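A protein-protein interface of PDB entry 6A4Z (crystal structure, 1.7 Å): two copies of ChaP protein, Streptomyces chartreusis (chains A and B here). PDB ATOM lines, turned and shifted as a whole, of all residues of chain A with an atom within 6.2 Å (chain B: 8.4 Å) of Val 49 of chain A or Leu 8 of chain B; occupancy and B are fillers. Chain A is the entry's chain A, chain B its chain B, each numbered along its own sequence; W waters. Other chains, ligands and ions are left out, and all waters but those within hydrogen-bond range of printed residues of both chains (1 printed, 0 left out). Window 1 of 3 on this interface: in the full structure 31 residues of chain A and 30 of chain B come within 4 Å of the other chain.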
ATOM      1  N   LEU A   8       6.845 -28.540   6.064  1.00  0.00           N
ATOM      2  CA  LEU A   8       6.322 -27.406   5.318  1.00  0.00           C
ATOM      3  C   LEU A   8       5.640 -27.931   4.060  1.00  0.00           C
ATOM      4  O   LEU A   8       6.277 -28.551   3.208  1.00  0.00           O
ATOM      5  CB  LEU A   8       7.426 -26.410   4.973  1.00  0.00           C
ATOM      6  CG  LEU A   8       6.971 -25.274   4.064  1.00  0.00           C
ATOM      7  CD1 LEU A   8       5.929 -24.369   4.741  1.00  0.00           C
ATOM      8  CD2 LEU A   8       8.172 -24.439   3.520  1.00  0.00           C
ATOM      9  N   ASN A   9       4.339 -27.708   3.950  1.00  0.00           N
ATOM     10  CA  ASN A   9       3.579 -28.296   2.858  1.00  0.00           C
ATOM     11  C   ASN A   9       3.410 -27.349   1.680  1.00  0.00           C
ATOM     12  O   ASN A   9       3.449 -27.786   0.526  1.00  0.00           O
ATOM     13  CB  ASN A   9       2.198 -28.745   3.368  1.00  0.00           C
ATOM     14  CG  ASN A   9       1.365 -29.390   2.292  1.00  0.00           C
ATOM     15  OD1 ASN A   9       0.538 -28.739   1.657  1.00  0.00           O
ATOM     16  ND2 ASN A   9       1.593 -30.675   2.062  1.00  0.00           N
ATOM     17  N   HIS A  10       3.187 -26.069   1.938  1.00  0.00           N
ATOM     18  CA  HIS A  10       3.143 -25.108   0.852  1.00  0.00           C
ATOM     19  C   HIS A  10       3.454 -23.725   1.392  1.00  0.00           C
ATOM     20  O   HIS A  10       3.383 -23.471   2.595  1.00  0.00           O
ATOM     21  CB  HIS A  10       1.810 -25.133   0.085  1.00  0.00           C
ATOM     22  CG  HIS A  10       0.581 -24.951   0.925  1.00  0.00           C
ATOM     23  ND1 HIS A  10      -0.099 -26.012   1.479  1.00  0.00           N
ATOM     24  CD2 HIS A  10      -0.121 -23.839   1.257  1.00  0.00           C
ATOM     25  CE1 HIS A  10      -1.158 -25.563   2.134  1.00  0.00           C
ATOM     26  NE2 HIS A  10      -1.199 -24.249   2.009  1.00  0.00           N
ATOM     27  N   THR A  11       3.877 -22.853   0.482  1.00  0.00           N
ATOM     28  CA  THR A  11       4.090 -21.460   0.810  1.00  0.00           C
ATOM     29  C   THR A  11       3.729 -20.643  -0.421  1.00  0.00           C
ATOM     30  O   THR A  11       3.883 -21.107  -1.554  1.00  0.00           O
ATOM     31  CB  THR A  11       5.522 -21.183   1.270  1.00  0.00           C
ATOM     32  OG1 THR A  11       5.612 -19.832   1.742  1.00  0.00           O
ATOM     33  CG2 THR A  11       6.508 -21.387   0.124  1.00  0.00           C
ATOM     34  N   LEU A  43       3.477 -24.926  -8.005  1.00  0.00           N
ATOM     35  CA  LEU A  43       4.706 -25.594  -8.431  1.00  0.00           C
ATOM     36  C   LEU A  43       5.080 -26.641  -7.386  1.00  0.00           C
ATOM     37  O   LEU A  43       5.426 -26.294  -6.254  1.00  0.00           O
ATOM     38  CB  LEU A  43       5.842 -24.586  -8.602  1.00  0.00           C
ATOM     39  CG  LEU A  43       7.142 -25.138  -9.195  1.00  0.00           C
ATOM     40  CD1 LEU A  43       6.973 -25.312 -10.689  1.00  0.00           C
ATOM     41  CD2 LEU A  43       8.324 -24.231  -8.893  1.00  0.00           C
ATOM     42  N   GLN A  44       5.059 -27.911  -7.778  1.00  0.00           N
ATOM     43  CA  GLN A  44       5.271 -29.016  -6.846  1.00  0.00           C
ATOM     44  C   GLN A  44       6.739 -29.434  -6.852  1.00  0.00           C
ATOM     45  O   GLN A  44       7.289 -29.775  -7.907  1.00  0.00           O
ATOM     46  CB  GLN A  44       4.379 -30.200  -7.209  1.00  0.00           C
ATOM     47  CG  GLN A  44       4.508 -31.382  -6.257  1.00  0.00           C
ATOM     48  CD  GLN A  44       4.128 -31.034  -4.834  1.00  0.00           C
ATOM     49  OE1 GLN A  44       3.063 -30.468  -4.585  1.00  0.00           O
ATOM     50  NE2 GLN A  44       4.996 -31.375  -3.890  1.00  0.00           N
ATOM     51  N   LEU A  45       7.380 -29.382  -5.689  1.00  0.00           N
ATOM     52  CA  LEU A  45       8.740 -29.880  -5.533  1.00  0.00           C
ATOM     53  C   LEU A  45       8.717 -31.309  -4.989  1.00  0.00           C
ATOM     54  O   LEU A  45       7.687 -31.828  -4.539  1.00  0.00           O
ATOM     55  CB  LEU A  45       9.565 -28.962  -4.624  1.00  0.00           C
ATOM     56  CG  LEU A  45       9.881 -27.532  -5.078  1.00  0.00           C
ATOM     57  CD1 LEU A  45      10.365 -27.485  -6.554  1.00  0.00           C
ATOM     58  CD2 LEU A  45       8.729 -26.568  -4.859  1.00  0.00           C
ATOM     59  N   ALA A  46       9.890 -31.945  -5.033  1.00  0.00           N
ATOM     60  CA  ALA A  46       9.985 -33.371  -4.752  1.00  0.00           C
ATOM     61  C   ALA A  46       9.829 -33.685  -3.273  1.00  0.00           C
ATOM     62  O   ALA A  46       9.418 -34.795  -2.928  1.00  0.00           O
ATOM     63  CB  ALA A  46      11.320 -33.910  -5.256  1.00  0.00           C
ATOM     64  N   ASN A  47      10.156 -32.748  -2.387  1.00  0.00           N
ATOM     65  CA  ASN A  47      10.127 -33.043  -0.955  1.00  0.00           C
ATOM     66  C   ASN A  47       8.801 -32.636  -0.307  1.00  0.00           C
ATOM     67  O   ASN A  47       8.776 -32.015   0.753  1.00  0.00           O
ATOM     68  CB  ASN A  47      11.314 -32.383  -0.264  1.00  0.00           C
ATOM     69  CG  ASN A  47      11.460 -30.927  -0.610  1.00  0.00           C
ATOM     70  OD1 ASN A  47      11.156 -30.494  -1.732  1.00  0.00           O
ATOM     71  ND2 ASN A  47      11.922 -30.143   0.357  1.00  0.00           N
ATOM     72  N   ASP A  48       7.688 -32.987  -0.964  1.00  0.00           N
ATOM     73  CA  ASP A  48       6.337 -32.860  -0.384  1.00  0.00           C
ATOM     74  C   ASP A  48       6.016 -31.416   0.000  1.00  0.00           C
ATOM     75  O   ASP A  48       5.382 -31.144   1.028  1.00  0.00           O
ATOM     76  CB  ASP A  48       6.170 -33.796   0.810  1.00  0.00           C
ATOM     77  CG  ASP A  48       6.179 -35.259   0.403  1.00  0.00           C
ATOM     78  OD1 ASP A  48       5.835 -35.550  -0.765  1.00  0.00           O
ATOM     79  OD2 ASP A  48       6.509 -36.115   1.255  1.00  0.00           O
ATOM     80  N   VAL A  49       6.449 -30.475  -0.839  1.00  0.00           N
ATOM     81  CA  VAL A  49       6.179 -29.057  -0.632  1.00  0.00           C
ATOM     82  C   VAL A  49       5.955 -28.408  -1.991  1.00  0.00           C
ATOM     83  O   VAL A  49       6.547 -28.807  -3.005  1.00  0.00           O
ATOM     84  CB  VAL A  49       7.318 -28.347   0.146  1.00  0.00           C
ATOM     85  CG1 VAL A  49       8.653 -28.446  -0.624  1.00  0.00           C
ATOM     86  CG2 VAL A  49       6.958 -26.893   0.442  1.00  0.00           C
ATOM     87  N   SER A  50       5.078 -27.413  -2.015  1.00  0.00           N
ATOM     88  CA  SER A  50       4.798 -26.671  -3.229  1.00  0.00           C
ATOM     89  C   SER A  50       4.994 -25.182  -2.990  1.00  0.00           C
ATOM     90  O   SER A  50       4.848 -24.681  -1.869  1.00  0.00           O
ATOM     91  CB  SER A  50       3.381 -26.940  -3.740  1.00  0.00           C
ATOM     92  OG  SER A  50       2.423 -26.434  -2.831  1.00  0.00           O
ATOM     93  N   ILE A  51       5.373 -24.488  -4.052  1.00  0.00           N
ATOM     94  CA  ILE A  51       5.352 -23.036  -4.083  1.00  0.00           C
ATOM     95  C   ILE A  51       4.104 -22.624  -4.843  1.00  0.00           C
ATOM     96  O   ILE A  51       3.951 -22.951  -6.026  1.00  0.00           O
ATOM     97  CB  ILE A  51       6.615 -22.462  -4.746  1.00  0.00           C
ATOM     98  CG1 ILE A  51       7.838 -22.732  -3.877  1.00  0.00           C
ATOM     99  CG2 ILE A  51       6.429 -20.959  -4.956  1.00  0.00           C
ATOM    100  CD1 ILE A  51       9.144 -22.310  -4.548  1.00  0.00           C
ATOM    101  N   CYS A  67      13.920 -18.255  -2.828  1.00  0.00           N
ATOM    102  CA  CYS A  67      13.666 -19.682  -2.760  1.00  0.00           C
ATOM    103  C   CYS A  67      14.895 -20.368  -3.317  1.00  0.00           C
ATOM    104  O   CYS A  67      15.426 -19.933  -4.329  1.00  0.00           O
ATOM    105  CB  CYS A  67      12.459 -20.130  -3.589  1.00  0.00           C
ATOM    106  SG  CYS A  67      10.910 -19.399  -3.069  1.00  0.00           S
ATOM    107  N   ALA A  68      15.336 -21.419  -2.659  1.00  0.00           N
ATOM    108  CA  ALA A  68      16.522 -22.142  -3.090  1.00  0.00           C
ATOM    109  C   ALA A  68      16.197 -23.617  -3.229  1.00  0.00           C
ATOM    110  O   ALA A  68      15.488 -24.188  -2.397  1.00  0.00           O
ATOM    111  CB  ALA A  68      17.650 -21.953  -2.105  1.00  0.00           C
ATOM    112  N   PHE A  69      16.747 -24.239  -4.266  1.00  0.00           N
ATOM    113  CA  PHE A  69      16.403 -25.597  -4.638  1.00  0.00           C
ATOM    114  C   PHE A  69      17.649 -26.468  -4.605  1.00  0.00           C
ATOM    115  O   PHE A  69      18.682 -26.100  -5.162  1.00  0.00           O
ATOM    116  CB  PHE A  69      15.754 -25.636  -6.020  1.00  0.00           C
ATOM    117  CG  PHE A  69      14.558 -24.755  -6.117  1.00  0.00           C
ATOM    118  CD1 PHE A  69      14.681 -23.433  -6.494  1.00  0.00           C
ATOM    119  CD2 PHE A  69      13.316 -25.241  -5.763  1.00  0.00           C
ATOM    120  CE1 PHE A  69      13.568 -22.587  -6.530  1.00  0.00           C
ATOM    121  CE2 PHE A  69      12.202 -24.410  -5.801  1.00  0.00           C
ATOM    122  CZ  PHE A  69      12.326 -23.091  -6.188  1.00  0.00           C
ATOM    123  N   LEU A  70      17.542 -27.603  -3.933  1.00  0.00           N
ATOM    124  CA  LEU A  70      18.607 -28.590  -3.868  1.00  0.00           C
ATOM    125  C   LEU A  70      18.382 -29.638  -4.951  1.00  0.00           C
ATOM    126  O   LEU A  70      17.337 -30.292  -4.985  1.00  0.00           O
ATOM    127  CB  LEU A  70      18.641 -29.257  -2.492  1.00  0.00           C
ATOM    128  CG  LEU A  70      19.770 -30.249  -2.236  1.00  0.00           C
ATOM    129  CD1 LEU A  70      21.111 -29.542  -2.291  1.00  0.00           C
ATOM    130  CD2 LEU A  70      19.581 -30.947  -0.899  1.00  0.00           C
ATOM    131  N   ALA B   5      14.097 -34.560  -9.598  1.00  0.00           N
ATOM    132  CA  ALA B   5      13.836 -34.602  -8.158  1.00  0.00           C
ATOM    133  C   ALA B   5      14.438 -33.339  -7.545  1.00  0.00           C
ATOM    134  O   ALA B   5      15.460 -33.342  -6.855  1.00  0.00           O
ATOM    135  CB  ALA B   5      14.401 -35.871  -7.537  1.00  0.00           C
ATOM    136  N   VAL B   6      13.762 -32.245  -7.824  1.00  0.00           N
ATOM    137  CA  VAL B   6      14.148 -30.929  -7.332  1.00  0.00           C
ATOM    138  C   VAL B   6      13.472 -30.699  -5.989  1.00  0.00           C
ATOM    139  O   VAL B   6      12.251 -30.831  -5.878  1.00  0.00           O
ATOM    140  CB  VAL B   6      13.752 -29.834  -8.335  1.00  0.00           C
ATOM    141  CG1 VAL B   6      14.042 -28.451  -7.756  1.00  0.00           C
ATOM    142  CG2 VAL B   6      14.480 -30.045  -9.670  1.00  0.00           C
ATOM    143  N   GLU B   7      14.255 -30.373  -4.966  1.00  0.00           N
ATOM    144  CA  GLU B   7      13.708 -30.084  -3.641  1.00  0.00           C
ATOM    145  C   GLU B   7      13.761 -28.596  -3.348  1.00  0.00           C
ATOM    146  O   GLU B   7      14.734 -27.927  -3.683  1.00  0.00           O
ATOM    147  CB  GLU B   7      14.478 -30.813  -2.541  1.00  0.00           C
ATOM    148  CG  GLU B   7      14.400 -32.313  -2.627  1.00  0.00           C
ATOM    149  CD  GLU B   7      15.197 -32.991  -1.529  1.00  0.00           C
ATOM    150  OE1 GLU B   7      15.049 -34.211  -1.358  1.00  0.00           O
ATOM    151  OE2 GLU B   7      15.975 -32.302  -0.837  1.00  0.00           O
ATOM    152  N   LEU B   8      12.734 -28.090  -2.667  1.00  0.00           N
ATOM    153  CA  LEU B   8      12.817 -26.764  -2.071  1.00  0.00           C
ATOM    154  C   LEU B   8      13.593 -26.891  -0.768  1.00  0.00           C
ATOM    155  O   LEU B   8      13.156 -27.592   0.151  1.00  0.00           O
ATOM    156  CB  LEU B   8      11.421 -26.197  -1.812  1.00  0.00           C
ATOM    157  CG  LEU B   8      11.454 -24.855  -1.066  1.00  0.00           C
ATOM    158  CD1 LEU B   8      12.137 -23.805  -1.907  1.00  0.00           C
ATOM    159  CD2 LEU B   8      10.031 -24.399  -0.683  1.00  0.00           C
ATOM    160  N   ASN B   9      14.749 -26.240  -0.694  1.00  0.00           N
ATOM    161  CA  ASN B   9      15.659 -26.396   0.433  1.00  0.00           C
ATOM    162  C   ASN B   9      15.505 -25.292   1.472  1.00  0.00           C
ATOM    163  O   ASN B   9      15.598 -25.565   2.671  1.00  0.00           O
ATOM    164  CB  ASN B   9      17.115 -26.415  -0.057  1.00  0.00           C
ATOM    165  CG  ASN B   9      18.097 -26.595   1.074  1.00  0.00           C
ATOM    166  OD1 ASN B   9      18.640 -25.624   1.604  1.00  0.00           O
ATOM    167  ND2 ASN B   9      18.320 -27.840   1.466  1.00  0.00           N
ATOM    168  N   HIS B  10      15.338 -24.051   1.033  1.00  0.00           N
ATOM    169  CA  HIS B  10      15.038 -22.988   1.979  1.00  0.00           C
ATOM    170  C   HIS B  10      14.305 -21.858   1.289  1.00  0.00           C
ATOM    171  O   HIS B  10      14.344 -21.696   0.067  1.00  0.00           O
ATOM    172  CB  HIS B  10      16.278 -22.458   2.706  1.00  0.00           C
ATOM    173  CG  HIS B  10      17.378 -21.972   1.814  1.00  0.00           C
ATOM    174  ND1 HIS B  10      18.348 -22.816   1.322  1.00  0.00           N
ATOM    175  CD2 HIS B  10      17.722 -20.725   1.408  1.00  0.00           C
ATOM    176  CE1 HIS B  10      19.223 -22.119   0.622  1.00  0.00           C
ATOM    177  NE2 HIS B  10      18.872 -20.849   0.660  1.00  0.00           N
ATOM    178  N   THR B  11      13.591 -21.093   2.112  1.00  0.00           N
ATOM    179  CA  THR B  11      12.896 -19.922   1.623  1.00  0.00           C
ATOM    180  C   THR B  11      12.947 -18.864   2.719  1.00  0.00           C
ATOM    181  O   THR B  11      12.929 -19.189   3.909  1.00  0.00           O
ATOM    182  CB  THR B  11      11.459 -20.280   1.219  1.00  0.00           C
ATOM    183  OG1 THR B  11      10.850 -19.167   0.555  1.00  0.00           O
ATOM    184  CG2 THR B  11      10.625 -20.675   2.446  1.00  0.00           C
ATOM    185  N   ILE B  12      13.049 -17.616   2.320  1.00  0.00           N
ATOM    186  CA  ILE B  12      13.124 -16.521   3.283  1.00  0.00           C
ATOM    187  C   ILE B  12      11.717 -16.041   3.578  1.00  0.00           C
ATOM    188  O   ILE B  12      10.885 -15.915   2.672  1.00  0.00           O
ATOM    189  CB  ILE B  12      14.004 -15.369   2.754  1.00  0.00           C
ATOM    190  CG1 ILE B  12      15.487 -15.750   2.844  1.00  0.00           C
ATOM    191  CG2 ILE B  12      13.729 -14.088   3.556  1.00  0.00           C
ATOM    192  CD1 ILE B  12      16.458 -14.742   2.179  1.00  0.00           C
ATOM    193  N   GLN B  44      13.773 -25.104  11.078  1.00  0.00           N
ATOM    194  CA  GLN B  44      14.017 -26.336  10.328  1.00  0.00           C
ATOM    195  C   GLN B  44      12.800 -27.254  10.360  1.00  0.00           C
ATOM    196  O   GLN B  44      12.401 -27.724  11.432  1.00  0.00           O
ATOM    197  CB  GLN B  44      15.236 -27.064  10.894  1.00  0.00           C
ATOM    198  CG  GLN B  44      15.620 -28.305  10.118  1.00  0.00           C
ATOM    199  CD  GLN B  44      16.010 -28.002   8.687  1.00  0.00           C
ATOM    200  OE1 GLN B  44      16.857 -27.145   8.429  1.00  0.00           O
ATOM    201  NE2 GLN B  44      15.377 -28.691   7.745  1.00  0.00           N
ATOM    202  N   LEU B  45      12.238 -27.547   9.187  1.00  0.00           N
ATOM    203  CA  LEU B  45      11.151 -28.514   9.093  1.00  0.00           C
ATOM    204  C   LEU B  45      11.692 -29.888   8.704  1.00  0.00           C
ATOM    205  O   LEU B  45      12.845 -30.043   8.282  1.00  0.00           O
ATOM    206  CB  LEU B  45      10.080 -28.063   8.091  1.00  0.00           C
ATOM    207  CG  LEU B  45       9.283 -26.785   8.390  1.00  0.00           C
ATOM    208  CD1 LEU B  45       8.833 -26.746   9.846  1.00  0.00           C
ATOM    209  CD2 LEU B  45      10.038 -25.519   8.027  1.00  0.00           C
ATOM    210  N   ASN B  47      10.845 -32.103   6.301  1.00  0.00           N
ATOM    211  CA  ASN B  47      10.966 -32.564   4.917  1.00  0.00           C
ATOM    212  C   ASN B  47      12.059 -31.805   4.163  1.00  0.00           C
ATOM    213  O   ASN B  47      11.872 -31.369   3.031  1.00  0.00           O
ATOM    214  CB  ASN B  47       9.624 -32.458   4.198  1.00  0.00           C
ATOM    215  CG  ASN B  47       8.981 -31.078   4.325  1.00  0.00           C
ATOM    216  OD1 ASN B  47       9.127 -30.387   5.340  1.00  0.00           O
ATOM    217  ND2 ASN B  47       8.258 -30.675   3.285  1.00  0.00           N
ATOM    218  N   ASP B  48      13.215 -31.661   4.818  1.00  0.00           N
ATOM    219  CA  ASP B  48      14.453 -31.161   4.203  1.00  0.00           C
ATOM    220  C   ASP B  48      14.296 -29.744   3.659  1.00  0.00           C
ATOM    221  O   ASP B  48      14.846 -29.396   2.608  1.00  0.00           O
ATOM    222  CB  ASP B  48      14.939 -32.114   3.108  1.00  0.00           C
ATOM    223  CG  ASP B  48      15.375 -33.455   3.667  1.00  0.00           C
ATOM    224  OD1 ASP B  48      15.775 -33.502   4.851  1.00  0.00           O
ATOM    225  OD2 ASP B  48      15.313 -34.455   2.928  1.00  0.00           O
ATOM    226  N   VAL B  49      13.567 -28.909   4.400  1.00  0.00           N
ATOM    227  CA  VAL B  49      13.364 -27.516   4.033  1.00  0.00           C
ATOM    228  C   VAL B  49      13.353 -26.676   5.302  1.00  0.00           C
ATOM    229  O   VAL B  49      12.910 -27.119   6.369  1.00  0.00           O
ATOM    230  CB  VAL B  49      12.065 -27.325   3.206  1.00  0.00           C
ATOM    231  CG1 VAL B  49      10.829 -27.790   3.999  1.00  0.00           C
ATOM    232  CG2 VAL B  49      11.922 -25.886   2.713  1.00  0.00           C
ATOM    233  N   SER B  50      13.871 -25.460   5.189  1.00  0.00           N
ATOM    234  CA  SER B  50      13.865 -24.530   6.306  1.00  0.00           C
ATOM    235  C   SER B  50      13.197 -23.233   5.879  1.00  0.00           C
ATOM    236  O   SER B  50      13.227 -22.856   4.708  1.00  0.00           O
ATOM    237  CB  SER B  50      15.293 -24.249   6.822  1.00  0.00           C
ATOM    238  OG  SER B  50      16.070 -23.518   5.879  1.00  0.00           O
ATOM    239  N   ILE B  51      12.552 -22.573   6.836  1.00  0.00           N
ATOM    240  CA  ILE B  51      12.088 -21.205   6.670  1.00  0.00           C
ATOM    241  C   ILE B  51      13.109 -20.314   7.343  1.00  0.00           C
ATOM    242  O   ILE B  51      13.377 -20.470   8.541  1.00  0.00           O
ATOM    243  CB  ILE B  51      10.699 -20.987   7.288  1.00  0.00           C
ATOM    244  CG1 ILE B  51       9.623 -21.702   6.473  1.00  0.00           C
ATOM    245  CG2 ILE B  51      10.430 -19.489   7.431  1.00  0.00           C
ATOM    246  CD1 ILE B  51       8.247 -21.634   7.147  1.00  0.00           C
ATOM    247  N   ALA B  68       2.158 -23.178   5.289  1.00  0.00           N
ATOM    248  CA  ALA B  68       1.276 -24.206   5.820  1.00  0.00           C
ATOM    249  C   ALA B  68       2.095 -25.432   6.170  1.00  0.00           C
ATOM    250  O   ALA B  68       3.015 -25.796   5.430  1.00  0.00           O
ATOM    251  CB  ALA B  68       0.213 -24.575   4.817  1.00  0.00           C
ATOM    252  N   LEU B  70       2.148 -29.536   7.413  1.00  0.00           N
ATOM    253  CA  LEU B  70       1.465 -30.818   7.493  1.00  0.00           C
ATOM    254  C   LEU B  70       1.986 -31.584   8.701  1.00  0.00           C
ATOM    255  O   LEU B  70       3.194 -31.794   8.841  1.00  0.00           O
ATOM    256  CB  LEU B  70       1.682 -31.626   6.210  1.00  0.00           C
ATOM    257  CG  LEU B  70       0.964 -32.978   6.077  1.00  0.00           C
ATOM    258  CD1 LEU B  70      -0.544 -32.786   6.087  1.00  0.00           C
ATOM    259  CD2 LEU B  70       1.374 -33.702   4.828  1.00  0.00           C
HETATM  260  O   HOH W   1       7.994 -18.349   1.029  1.00  0.00           O
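Leu 8 of chain A touches Leu 45 of chain B, and with the chains exchanged Leu 45 of chain A touches Leu 8 of chain B. Leu 8 of chain A touches Asn 47 of chain B, and with the chains exchanged Asn 47 of chain A touches Leu 8 of chain B. Asn 9 of chain A touches Ala 68 of chain B, and with the chains exchanged Ala 68 of chain A touches Asn 9 of chain B. Asn 47 of chain A touches its own counterpart, Asn 47 of chain B. Of the 25 pairs that touch across the chains among the printed residues, 15 have their exchanged pair printed and touching as well.
ND2 of Asn 47 of chain A lies within hydrogen-bond range of O of Leu 8 of chain B (2.8 Å). ND2 of Asn 47 of chain B is in hydrogen-bond range of O of Asn 47 of chain A, 2.9 Å away. O of Leu 8 of chain A sits at hydrogen-bond distance from ND2 of Asn 47 of chain B, at 2.9 Å. The backbone NH of Ala 46 of chain A sits at hydrogen-bond distance from the backbone carbonyl oxygen of Val 6 of chain B (2.7 Å). The backbone carbonyl oxygen (O) of Glu 7 of chain B is in hydrogen-bond range of the backbone NH (N) of Leu 70 of chain A, at 2.8 Å. The backbone carbonyl oxygen (O) of His 10 of chain A sits at hydrogen-bond distance from the backbone NH (N) of Ala 68 of chain B, at 3.0 Å. The backbone NH (N) of Asn 9 of chain A sits at hydrogen-bond distance from the backbone carbonyl oxygen (O) of Ala 68 of chain B (2.8 Å). The side-chain sulfur (SG) of Cys 67 of chain A is in hydrogen-bond range of the side-chain hydroxyl (OG1) of Thr 11 of chain B (3.6 Å). The backbone carbonyl oxygen (O) of His 10 of chain B lies within hydrogen-bond range of the backbone NH (N) of Ala 68 of chain A (2.9 Å). The backbone carbonyl oxygen of Ala 68 of chain A is in hydrogen-bond range of the backbone NH of Asn 9 of chain B (2.8 Å).
Water W1 lies within hydrogen-bond range of OG1 of Thr 11 of chain A and OG1 of Thr 11 of chain B.
Printed residues of chain B within 4 Å of Asn 9 of chain A: Ala 68. Of the printed residues of chain B, Asp 48 of chain A touches Asn 47. Printed residues of chain B within 4 Å of Val 49 of chain A: Leu 8 (3.8 Å). Of chain A, only Leu 45, Asn 47, Val 49, Ala 68 and Phe 69 come within 4 Å of Leu 8 of chain B. The nearest printed residue of chain A that does not touch Ala 5 of chain B is Leu 70 of chain A (4.04 Å).
Among the printed residues, pairs that only touch across the chains: Leu 8 of chain A with Leu 45 of chain B (3.8 Å), Leu 8 of chain A with Val 49 of chain B (3.8 Å), Leu 8 of chain A with Ala 68 of chain B (3.3 Å), Leu 45 of chain A with Val 6 of chain B (3.5 Å), Leu 45 of chain A with Leu 8 of chain B (3.8 Å), Ala 46 of chain A with Ala 5 of chain B (3.9 Å), Asn 47 of chain A with Glu 7 of chain B (3.2 Å), Asn 47 of chain A with Asp 48 of chain B (3.8 Å), Asp 48 of chain A with Asn 47 of chain B (3.7 Å), Val 49 of chain A with Leu 8 of chain B (3.8 Å), Cys 67 of chain A with His 10 of chain B (3.5 Å), Ala 68 of chain A with Leu 8 of chain B (3.4 Å), Phe 69 of chain A with Val 6 of chain B (3.7 Å), Phe 69 of chain A with Glu 7 of chain B (3.0 Å) and Phe 69 of chain A with Leu 8 of chain B (3.9 Å).
The side-chain amide nitrogen of Gln 44 of chain B sits at hydrogen-bond distance from the backbone carbonyl oxygen of Val 49 of chain B (3.2 Å). OD1 of Asn 9 of chain A lies within hydrogen-bond range of ND1 of His 10 of chain A. The backbone carbonyl oxygen (O) of Asn 9 of chain B is in hydrogen-bond range of the backbone NH (N) of Ser 50 of chain B (3.1 Å). The backbone NH of Ser 50 of chain A sits at hydrogen-bond distance from the backbone carbonyl oxygen of Asn 9 of chain A, at 3.0 Å. OD1 of Asn 9 of chain B is in hydrogen-bond range of ND1 of His 10 of chain B (2.8 Å). The backbone carbonyl oxygen (O) of Ser 50 of chain B is in hydrogen-bond range of the backbone NH (N) of Thr 11 of chain B (3.2 Å).
Printed residues of chain A that touch a printed residue of chain B: Leu 8, Asn 9, His 10, Leu 45, Ala 46, Asn 47, Asp 48, Val 49, Cys 67, Ala 68, Phe 69 and Leu 70. Hydrophobic or aromatic side chains of chain A that line the printed part of chain B: Leu 8, His 10, Leu 45, Ala 46, Val 49, Ala 68, Phe 69 and Leu 70. Hydrophobic or aromatic side chains of chain B within 4 Å of the printed part of chain A: Val 6, Leu 8, His 10, Leu 45, Val 49 and Ala 68. Among the printed residues, no Asp or Glu carboxylate lies within 4 Å of a Lys or Arg side-chain nitrogen of the other chain.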
